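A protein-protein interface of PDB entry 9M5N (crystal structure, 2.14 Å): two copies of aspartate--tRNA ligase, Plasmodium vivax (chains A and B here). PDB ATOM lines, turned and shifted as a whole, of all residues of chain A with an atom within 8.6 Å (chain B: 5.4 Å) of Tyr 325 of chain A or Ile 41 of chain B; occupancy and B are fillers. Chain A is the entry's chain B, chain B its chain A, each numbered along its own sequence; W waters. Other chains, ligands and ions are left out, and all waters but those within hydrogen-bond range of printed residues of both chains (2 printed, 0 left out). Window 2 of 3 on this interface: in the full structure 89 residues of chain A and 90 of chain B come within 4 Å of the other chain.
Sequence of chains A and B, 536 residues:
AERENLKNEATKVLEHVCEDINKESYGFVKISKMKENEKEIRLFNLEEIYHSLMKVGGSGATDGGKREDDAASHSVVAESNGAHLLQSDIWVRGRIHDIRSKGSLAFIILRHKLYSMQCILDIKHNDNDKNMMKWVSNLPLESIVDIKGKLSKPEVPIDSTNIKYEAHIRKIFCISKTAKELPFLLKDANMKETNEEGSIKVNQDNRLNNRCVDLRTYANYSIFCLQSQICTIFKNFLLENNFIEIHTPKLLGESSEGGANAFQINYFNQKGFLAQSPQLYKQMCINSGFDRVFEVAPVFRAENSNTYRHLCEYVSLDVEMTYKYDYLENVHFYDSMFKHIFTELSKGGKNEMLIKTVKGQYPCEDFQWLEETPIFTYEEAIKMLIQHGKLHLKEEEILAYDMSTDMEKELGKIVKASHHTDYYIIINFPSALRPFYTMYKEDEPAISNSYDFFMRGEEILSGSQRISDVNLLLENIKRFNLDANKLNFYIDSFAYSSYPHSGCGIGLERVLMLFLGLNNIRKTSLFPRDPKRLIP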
ATOM      1  N   THR A 322      -6.484 -23.264 -13.086  1.00  0.00           N
ATOM      2  CA  THR A 322      -5.383 -23.449 -12.185  1.00  0.00           C
ATOM      3  C   THR A 322      -4.332 -24.359 -12.793  1.00  0.00           C
ATOM      4  O   THR A 322      -4.592 -25.013 -13.749  1.00  0.00           O
ATOM      5  CB  THR A 322      -5.839 -24.092 -10.874  1.00  0.00           C
ATOM      6  OG1 THR A 322      -6.481 -25.326 -11.139  1.00  0.00           O
ATOM      7  CG2 THR A 322      -6.793 -23.216 -10.176  1.00  0.00           C
ATOM      8  N   TYR A 323      -3.141 -24.349 -12.226  1.00  0.00           N
ATOM      9  CA  TYR A 323      -2.056 -25.216 -12.624  1.00  0.00           C
ATOM     10  C   TYR A 323      -1.394 -25.774 -11.382  1.00  0.00           C
ATOM     11  O   TYR A 323      -1.538 -25.234 -10.325  1.00  0.00           O
ATOM     12  CB  TYR A 323      -1.050 -24.553 -13.556  1.00  0.00           C
ATOM     13  CG  TYR A 323      -0.313 -23.370 -13.030  1.00  0.00           C
ATOM     14  CD1 TYR A 323       0.845 -23.516 -12.334  1.00  0.00           C
ATOM     15  CD2 TYR A 323      -0.761 -22.104 -13.273  1.00  0.00           C
ATOM     16  CE1 TYR A 323       1.524 -22.429 -11.870  1.00  0.00           C
ATOM     17  CE2 TYR A 323      -0.098 -21.018 -12.806  1.00  0.00           C
ATOM     18  CZ  TYR A 323       1.041 -21.193 -12.107  1.00  0.00           C
ATOM     19  OH  TYR A 323       1.697 -20.122 -11.651  1.00  0.00           O
ATOM     20  N   LYS A 324      -0.694 -26.877 -11.501  1.00  0.00           N
ATOM     21  CA  LYS A 324      -0.070 -27.470 -10.345  1.00  0.00           C
ATOM     22  C   LYS A 324       1.195 -26.788  -9.944  1.00  0.00           C
ATOM     23  O   LYS A 324       1.246 -26.165  -8.925  1.00  0.00           O
ATOM     24  CB  LYS A 324       0.175 -28.943 -10.558  1.00  0.00           C
ATOM     25  CG  LYS A 324      -1.092 -29.748 -10.616  1.00  0.00           C
ATOM     26  CD  LYS A 324      -0.887 -31.046 -11.344  1.00  0.00           C
ATOM     27  CE  LYS A 324      -2.107 -31.919 -11.216  1.00  0.00           C
ATOM     28  NZ  LYS A 324      -2.034 -33.120 -12.072  1.00  0.00           N
ATOM     29  N   TYR A 325       2.241 -26.965 -10.719  1.00  0.00           N
ATOM     30  CA  TYR A 325       3.504 -26.341 -10.408  1.00  0.00           C
ATOM     31  C   TYR A 325       4.067 -25.441 -11.467  1.00  0.00           C
ATOM     32  O   TYR A 325       4.839 -24.579 -11.172  1.00  0.00           O
ATOM     33  CB  TYR A 325       4.523 -27.408 -10.075  1.00  0.00           C
ATOM     34  CG  TYR A 325       4.090 -28.253  -8.941  1.00  0.00           C
ATOM     35  CD1 TYR A 325       4.184 -27.803  -7.666  1.00  0.00           C
ATOM     36  CD2 TYR A 325       3.534 -29.470  -9.156  1.00  0.00           C
ATOM     37  CE1 TYR A 325       3.762 -28.560  -6.621  1.00  0.00           C
ATOM     38  CE2 TYR A 325       3.115 -30.241  -8.119  1.00  0.00           C
ATOM     39  CZ  TYR A 325       3.235 -29.770  -6.853  1.00  0.00           C
ATOM     40  OH  TYR A 325       2.811 -30.517  -5.823  1.00  0.00           O
ATOM     41  N   ASP A 326       3.685 -25.660 -12.708  1.00  0.00           N
ATOM     42  CA  ASP A 326       4.212 -24.889 -13.811  1.00  0.00           C
ATOM     43  C   ASP A 326       3.115 -24.382 -14.694  1.00  0.00           C
ATOM     44  O   ASP A 326       2.265 -25.115 -15.074  1.00  0.00           O
ATOM     45  CB  ASP A 326       5.139 -25.787 -14.607  1.00  0.00           C
ATOM     46  CG  ASP A 326       5.962 -25.056 -15.631  1.00  0.00           C
ATOM     47  OD1 ASP A 326       6.948 -25.631 -16.060  1.00  0.00           O
ATOM     48  OD2 ASP A 326       5.663 -23.945 -16.026  1.00  0.00           O
ATOM     49  N   TYR A 327       3.177 -23.127 -15.101  1.00  0.00           N
ATOM     50  CA  TYR A 327       2.180 -22.527 -15.985  1.00  0.00           C
ATOM     51  C   TYR A 327       2.132 -23.119 -17.392  1.00  0.00           C
ATOM     52  O   TYR A 327       1.132 -23.053 -18.042  1.00  0.00           O
ATOM     53  CB  TYR A 327       2.283 -21.018 -16.045  1.00  0.00           C
ATOM     54  CG  TYR A 327       3.212 -20.535 -17.093  1.00  0.00           C
ATOM     55  CD1 TYR A 327       2.746 -20.041 -18.272  1.00  0.00           C
ATOM     56  CD2 TYR A 327       4.558 -20.590 -16.904  1.00  0.00           C
ATOM     57  CE1 TYR A 327       3.599 -19.609 -19.233  1.00  0.00           C
ATOM     58  CE2 TYR A 327       5.419 -20.155 -17.862  1.00  0.00           C
ATOM     59  CZ  TYR A 327       4.924 -19.669 -19.022  1.00  0.00           C
ATOM     60  OH  TYR A 327       5.772 -19.246 -19.967  1.00  0.00           O
ATOM     61  N   LEU A 328       3.204 -23.765 -17.831  1.00  0.00           N
ATOM     62  CA  LEU A 328       3.288 -24.448 -19.100  1.00  0.00           C
ATOM     63  C   LEU A 328       2.243 -25.551 -19.222  1.00  0.00           C
ATOM     64  O   LEU A 328       1.851 -25.843 -20.313  1.00  0.00           O
ATOM     65  CB  LEU A 328       4.696 -24.953 -19.346  1.00  0.00           C
ATOM     66  CG  LEU A 328       5.617 -23.773 -19.577  1.00  0.00           C
ATOM     67  CD1 LEU A 328       7.071 -24.146 -19.677  1.00  0.00           C
ATOM     68  CD2 LEU A 328       5.186 -22.961 -20.771  1.00  0.00           C
ATOM     69  N   GLU A 329       1.892 -26.221 -18.126  1.00  0.00           N
ATOM     70  CA  GLU A 329       0.819 -27.174 -18.081  1.00  0.00           C
ATOM     71  C   GLU A 329      -0.401 -26.577 -18.761  1.00  0.00           C
ATOM     72  O   GLU A 329      -1.006 -27.195 -19.578  1.00  0.00           O
ATOM     73  CB  GLU A 329       0.437 -27.478 -16.636  1.00  0.00           C
ATOM     74  CG  GLU A 329       1.483 -28.157 -15.779  1.00  0.00           C
ATOM     75  CD  GLU A 329       1.202 -28.049 -14.293  1.00  0.00           C
ATOM     76  OE1 GLU A 329       0.049 -28.035 -13.898  1.00  0.00           O
ATOM     77  OE2 GLU A 329       2.151 -27.964 -13.524  1.00  0.00           O
ATOM     78  N   ASN A 330      -0.761 -25.363 -18.404  1.00  0.00           N
ATOM     79  CA  ASN A 330      -1.920 -24.724 -19.006  1.00  0.00           C
ATOM     80  C   ASN A 330      -1.659 -24.376 -20.471  1.00  0.00           C
ATOM     81  O   ASN A 330      -2.557 -24.512 -21.313  1.00  0.00           O
ATOM     82  CB  ASN A 330      -2.274 -23.466 -18.215  1.00  0.00           C
ATOM     83  CG  ASN A 330      -2.766 -23.751 -16.803  1.00  0.00           C
ATOM     84  OD1 ASN A 330      -2.885 -22.826 -16.012  1.00  0.00           O
ATOM     85  ND2 ASN A 330      -3.079 -25.017 -16.487  1.00  0.00           N
ATOM     86  N   ASN A 449       5.828 -14.631 -17.904  1.00  0.00           N
ATOM     87  CA  ASN A 449       5.283 -15.931 -18.278  1.00  0.00           C
ATOM     88  C   ASN A 449       3.969 -15.682 -19.011  1.00  0.00           C
ATOM     89  O   ASN A 449       2.869 -15.784 -18.454  1.00  0.00           O
ATOM     90  CB  ASN A 449       5.125 -16.808 -17.054  1.00  0.00           C
ATOM     91  CG  ASN A 449       6.455 -17.221 -16.494  1.00  0.00           C
ATOM     92  OD1 ASN A 449       7.459 -17.239 -17.207  1.00  0.00           O
ATOM     93  ND2 ASN A 449       6.480 -17.559 -15.218  1.00  0.00           N
ATOM     94  N   GLN A 465       0.378 -16.558 -17.268  1.00  0.00           N
ATOM     95  CA  GLN A 465       0.391 -16.852 -15.842  1.00  0.00           C
ATOM     96  C   GLN A 465      -0.029 -15.587 -15.096  1.00  0.00           C
ATOM     97  O   GLN A 465       0.419 -14.488 -15.430  1.00  0.00           O
ATOM     98  CB  GLN A 465       1.798 -17.296 -15.372  1.00  0.00           C
ATOM     99  CG  GLN A 465       1.871 -17.676 -13.859  1.00  0.00           C
ATOM    100  CD  GLN A 465       3.298 -17.967 -13.338  1.00  0.00           C
ATOM    101  OE1 GLN A 465       4.125 -18.556 -14.021  1.00  0.00           O
ATOM    102  NE2 GLN A 465       3.566 -17.567 -12.116  1.00  0.00           N
ATOM    103  N   PRO A 500      -2.368 -20.976  -7.842  1.00  0.00           N
ATOM    104  CA  PRO A 500      -1.633 -20.663  -9.078  1.00  0.00           C
ATOM    105  C   PRO A 500      -2.570 -20.827 -10.267  1.00  0.00           C
ATOM    106  O   PRO A 500      -3.253 -21.840 -10.399  1.00  0.00           O
ATOM    107  CB  PRO A 500      -0.484 -21.679  -9.095  1.00  0.00           C
ATOM    108  CG  PRO A 500      -0.732 -22.626  -7.945  1.00  0.00           C
ATOM    109  CD  PRO A 500      -1.686 -21.974  -7.001  1.00  0.00           C
ATOM    110  N   ILE B  21      12.151 -28.908   0.733  1.00  0.00           N
ATOM    111  CA  ILE B  21      11.078 -29.807   1.148  1.00  0.00           C
ATOM    112  C   ILE B  21      11.543 -31.243   1.326  1.00  0.00           C
ATOM    113  O   ILE B  21      10.811 -32.046   1.915  1.00  0.00           O
ATOM    114  CB  ILE B  21       9.900 -29.798   0.151  1.00  0.00           C
ATOM    115  CG1 ILE B  21      10.337 -30.384  -1.190  1.00  0.00           C
ATOM    116  CG2 ILE B  21       9.349 -28.383  -0.038  1.00  0.00           C
ATOM    117  CD1 ILE B  21       9.183 -30.646  -2.131  1.00  0.00           C
ATOM    118  N   ILE B  31       6.194 -22.054  -5.172  1.00  0.00           N
ATOM    119  CA  ILE B  31       5.826 -23.138  -6.076  1.00  0.00           C
ATOM    120  C   ILE B  31       7.059 -23.697  -6.780  1.00  0.00           C
ATOM    121  O   ILE B  31       7.162 -24.912  -7.003  1.00  0.00           O
ATOM    122  CB  ILE B  31       4.769 -22.643  -7.082  1.00  0.00           C
ATOM    123  CG1 ILE B  31       3.416 -22.536  -6.399  1.00  0.00           C
ATOM    124  CG2 ILE B  31       4.649 -23.597  -8.248  1.00  0.00           C
ATOM    125  CD1 ILE B  31       2.885 -23.880  -5.997  1.00  0.00           C
ATOM    126  N   MET B  34       8.780 -26.767  -5.016  1.00  0.00           N
ATOM    127  CA  MET B  34       8.063 -28.011  -4.733  1.00  0.00           C
ATOM    128  C   MET B  34       8.533 -29.115  -5.687  1.00  0.00           C
ATOM    129  O   MET B  34       7.790 -29.628  -6.520  1.00  0.00           O
ATOM    130  CB  MET B  34       6.562 -27.787  -4.830  1.00  0.00           C
ATOM    131  CG  MET B  34       5.986 -26.827  -3.788  1.00  0.00           C
ATOM    132  SD  MET B  34       6.031 -27.542  -2.127  1.00  0.00           S
ATOM    133  CE  MET B  34       4.670 -28.688  -2.205  1.00  0.00           C
ATOM    134  N   LYS B  35       9.764 -29.535  -5.489  1.00  0.00           N
ATOM    135  CA  LYS B  35      10.359 -30.603  -6.251  1.00  0.00           C
ATOM    136  C   LYS B  35      10.852 -31.610  -5.241  1.00  0.00           C
ATOM    137  O   LYS B  35      11.631 -31.267  -4.388  1.00  0.00           O
ATOM    138  CB  LYS B  35      11.544 -30.079  -7.043  1.00  0.00           C
ATOM    139  CG  LYS B  35      11.189 -29.409  -8.350  1.00  0.00           C
ATOM    140  N   GLU B  36      10.410 -32.852  -5.332  1.00  0.00           N
ATOM    141  CA  GLU B  36      10.850 -33.861  -4.390  1.00  0.00           C
ATOM    142  C   GLU B  36      11.953 -34.647  -5.057  1.00  0.00           C
ATOM    143  O   GLU B  36      11.732 -35.302  -6.056  1.00  0.00           O
ATOM    144  CB  GLU B  36       9.693 -34.774  -4.010  1.00  0.00           C
ATOM    145  CG  GLU B  36       9.773 -35.344  -2.613  1.00  0.00           C
ATOM    146  CD  GLU B  36       8.525 -36.086  -2.204  1.00  0.00           C
ATOM    147  OE1 GLU B  36       8.305 -36.283  -1.007  1.00  0.00           O
ATOM    148  OE2 GLU B  36       7.762 -36.483  -3.070  1.00  0.00           O
ATOM    149  N   LYS B  39      12.587 -34.178  -8.826  1.00  0.00           N
ATOM    150  CA  LYS B  39      11.609 -34.702  -9.744  1.00  0.00           C
ATOM    151  C   LYS B  39      10.264 -34.047  -9.477  1.00  0.00           C
ATOM    152  O   LYS B  39      10.147 -33.192  -8.614  1.00  0.00           O
ATOM    153  CB  LYS B  39      11.522 -36.212  -9.626  1.00  0.00           C
ATOM    154  N   GLU B  40       9.242 -34.487 -10.187  1.00  0.00           N
ATOM    155  CA  GLU B  40       7.933 -33.853 -10.079  1.00  0.00           C
ATOM    156  C   GLU B  40       7.011 -34.672  -9.184  1.00  0.00           C
ATOM    157  O   GLU B  40       6.979 -35.905  -9.259  1.00  0.00           O
ATOM    158  CB  GLU B  40       7.285 -33.664 -11.455  1.00  0.00           C
ATOM    159  CG  GLU B  40       6.106 -32.678 -11.455  1.00  0.00           C
ATOM    160  CD  GLU B  40       5.362 -32.632 -12.788  1.00  0.00           C
ATOM    161  OE1 GLU B  40       4.247 -32.058 -12.843  1.00  0.00           O
ATOM    162  OE2 GLU B  40       5.892 -33.171 -13.783  1.00  0.00           O
ATOM    163  N   ILE B  41       6.255 -33.965  -8.347  1.00  0.00           N
ATOM    164  CA  ILE B  41       5.275 -34.572  -7.452  1.00  0.00           C
ATOM    165  C   ILE B  41       4.042 -34.984  -8.248  1.00  0.00           C
ATOM    166  O   ILE B  41       3.537 -34.213  -9.071  1.00  0.00           O
ATOM    167  CB  ILE B  41       4.897 -33.581  -6.339  1.00  0.00           C
ATOM    168  CG1 ILE B  41       6.044 -33.436  -5.333  1.00  0.00           C
ATOM    169  CG2 ILE B  41       3.582 -33.975  -5.685  1.00  0.00           C
ATOM    170  CD1 ILE B  41       5.958 -32.175  -4.481  1.00  0.00           C
ATOM    171  N   ARG B  42       3.536 -36.189  -8.003  1.00  0.00           N
ATOM    172  CA  ARG B  42       2.194 -36.513  -8.486  1.00  0.00           C
ATOM    173  C   ARG B  42       1.185 -35.969  -7.481  1.00  0.00           C
ATOM    174  O   ARG B  42       0.940 -36.576  -6.433  1.00  0.00           O
ATOM    175  CB  ARG B  42       2.002 -38.009  -8.690  1.00  0.00           C
ATOM    176  CG  ARG B  42       0.625 -38.302  -9.294  1.00  0.00           C
ATOM    177  CD  ARG B  42       0.463 -39.745  -9.701  1.00  0.00           C
ATOM    178  NE  ARG B  42      -0.870 -40.008 -10.239  1.00  0.00           N
ATOM    179  N   LEU B  43       0.591 -34.828  -7.817  1.00  0.00           N
ATOM    180  CA  LEU B  43      -0.285 -34.074  -6.930  1.00  0.00           C
ATOM    181  C   LEU B  43      -1.741 -34.411  -7.225  1.00  0.00           C
ATOM    182  O   LEU B  43      -2.171 -34.336  -8.377  1.00  0.00           O
ATOM    183  CB  LEU B  43      -0.040 -32.575  -7.114  1.00  0.00           C
ATOM    184  CG  LEU B  43      -0.883 -31.626  -6.270  1.00  0.00           C
ATOM    185  CD1 LEU B  43      -0.563 -31.835  -4.790  1.00  0.00           C
ATOM    186  CD2 LEU B  43      -0.664 -30.172  -6.695  1.00  0.00           C
ATOM    187  N   TRP B  91       0.486 -36.991  -2.253  1.00  0.00           N
ATOM    188  CA  TRP B  91       0.387 -35.549  -2.133  1.00  0.00           C
ATOM    189  C   TRP B  91      -1.003 -35.093  -2.554  1.00  0.00           C
ATOM    190  O   TRP B  91      -1.537 -35.549  -3.575  1.00  0.00           O
ATOM    191  CB  TRP B  91       1.429 -34.863  -3.004  1.00  0.00           C
ATOM    192  CG  TRP B  91       2.821 -34.977  -2.520  1.00  0.00           C
ATOM    193  CD1 TRP B  91       3.697 -35.987  -2.772  1.00  0.00           C
ATOM    194  CD2 TRP B  91       3.522 -34.027  -1.707  1.00  0.00           C
ATOM    195  NE1 TRP B  91       4.908 -35.727  -2.164  1.00  0.00           N
ATOM    196  CE2 TRP B  91       4.824 -34.529  -1.505  1.00  0.00           C
ATOM    197  CE3 TRP B  91       3.174 -32.797  -1.132  1.00  0.00           C
ATOM    198  CZ2 TRP B  91       5.778 -33.845  -0.759  1.00  0.00           C
ATOM    199  CZ3 TRP B  91       4.118 -32.123  -0.399  1.00  0.00           C
ATOM    200  CH2 TRP B  91       5.406 -32.648  -0.213  1.00  0.00           C
ATOM    201  N   ARG B  93      -3.468 -31.343  -2.653  1.00  0.00           N
ATOM    202  CA  ARG B  93      -3.574 -29.901  -2.455  1.00  0.00           C
ATOM    203  C   ARG B  93      -5.000 -29.551  -2.050  1.00  0.00           C
ATOM    204  O   ARG B  93      -5.944 -30.218  -2.471  1.00  0.00           O
ATOM    205  CB  ARG B  93      -3.182 -29.132  -3.724  1.00  0.00           C
ATOM    206  CG  ARG B  93      -3.462 -27.632  -3.686  1.00  0.00           C
ATOM    207  CD  ARG B  93      -2.806 -26.897  -4.884  1.00  0.00           C
ATOM    208  NE  ARG B  93      -1.362 -27.100  -4.890  1.00  0.00           N
ATOM    209  CZ  ARG B  93      -0.549 -26.730  -5.868  1.00  0.00           C
ATOM    210  NH1 ARG B  93      -0.996 -26.076  -6.928  1.00  0.00           N
ATOM    211  NH2 ARG B  93       0.743 -27.023  -5.782  1.00  0.00           N
ATOM    212  N   ASP B 146      -0.242 -27.908   0.315  1.00  0.00           N
ATOM    213  CA  ASP B 146       0.075 -29.227  -0.213  1.00  0.00           C
ATOM    214  C   ASP B 146       0.458 -30.111   0.963  1.00  0.00           C
ATOM    215  O   ASP B 146       1.402 -29.799   1.694  1.00  0.00           O
ATOM    216  CB  ASP B 146       1.215 -29.170  -1.235  1.00  0.00           C
ATOM    217  CG  ASP B 146       0.802 -28.506  -2.543  1.00  0.00           C
ATOM    218  OD1 ASP B 146      -0.394 -28.168  -2.677  1.00  0.00           O
ATOM    219  OD2 ASP B 146       1.665 -28.315  -3.430  1.00  0.00           O
HETATM  220  O   HOH W   1      -3.670 -25.316  -7.954  1.00  0.00           O
HETATM  221  O   HOH W   2       4.363 -29.124 -13.843  1.00  0.00           O
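The side-chain amide nitrogen (NE2) of Gln 465 of chain A sits close to the side-chain hydroxyl (OH) of Tyr 323 of chain A, 3.2 Å away.
The backbone NH of Tyr 325 of chain A lies within hydrogen-bond range of the side-chain carboxylate of Glu 329 of chain A.
The backbone carbonyl oxygen (O) of Pro 500 of chain A is in hydrogen-bond range of the backbone NH (N) of Tyr 323 of chain A, at 3.1 Å.
NE of Arg 93 of chain B lies within salt-bridge range of OD1 of Asp 146 of chain B (2.6 Å).
N of Lys 324 of chain A is in hydrogen-bond range of OE1 of Glu 329 of chain A, at 2.8 Å.
OD2 of Asp 146 of chain B is in hydrogen-bond range of OH of Tyr 325 of chain A (3.4 Å).
NH1 of Arg 93 of chain B sits at hydrogen-bond distance from O of Lys 324 of chain A (3.0 Å).
No position is printed for both chains.
Of the 10 pairs that touch across the chains among the printed residues, none has its exchanged pair printed and touching as well.
Of the printed residues of chain B, Tyr 325 of chain A touches Ile 31, Met 34, Ile 41, Leu 43, Arg 93 and Asp 146.
Ile 41 of chain B touches one residue of chain A.
Of the printed residues of chain A, Asp 146 of chain B touches Tyr 325.
Printed residues of chain A within 4 Å of Arg 93 of chain B: Tyr 323, Lys 324, Tyr 325 and Pro 500.
Printed residues of chain A within 4 Å of Ile 31 of chain B: Tyr 325 (3.1 Å).
Of the printed residues of chain A, Leu 43 of chain B touches Lys 324 (3.7 Å) and Tyr 325 (3.6 Å).
Printed residues of chain A within 4 Å of Met 34 of chain B: Tyr 325 (3.4 Å).
Gln 465 of chain A touches none of the printed residues of chain B.
Water W2 lies within hydrogen-bond range of OE2 of Glu 329 of chain A (2.5 Å) and OE1 of Glu 40 of chain B (3.1 Å).
Water W1 bridges the guanidinium group of Arg 93 of chain B (3.0 Å) and the backbone carbonyl oxygen of Tyr 323 of chain A (3.2 Å).
Printed residues of chain B that touch a printed residue of chain A: Ile 31, Met 34, Ile 41, Leu 43, Arg 93 and Asp 146.
Hydrophobic or aromatic side chains of chain B that line the printed part of chain A: Ile 31, Met 34, Ile 41 and Leu 43.
Of the 12 printed residues of chain A, 4 touch a printed residue of chain B.
Printed residues of chain A that touch a printed residue of chain B: Tyr 323, Lys 324, Tyr 325 and Pro 500.
Hydrophobic or aromatic side chains of chain A within 4 Å of the printed part of chain B: Tyr 325 and Pro 500.
Among the printed residues, 10 pairs touch across the chains.
Among the printed residues, no Asp or Glu carboxylate lies within 4 Å of a Lys or Arg side-chain nitrogen of the other chain.
Among the printed residues, pairs that only touch across the chains: Tyr 325 of chain A with Ile 31 of chain B (3.1 Å), Tyr 325 of chain A with Met 34 of chain B (3.4 Å), Tyr 325 of chain A with Arg 93 of chain B (3.5 Å), Tyr 323 of chain A with Arg 93 of chain B (3.5 Å), Tyr 325 of chain A with Ile 41 of chain B (3.5 Å), Tyr 325 of chain A with Leu 43 of chain B (3.6 Å), Pro 500 of chain A with Arg 93 of chain B (3.6 Å) and Lys 324 of chain A with Leu 43 of chain B (3.7 Å).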
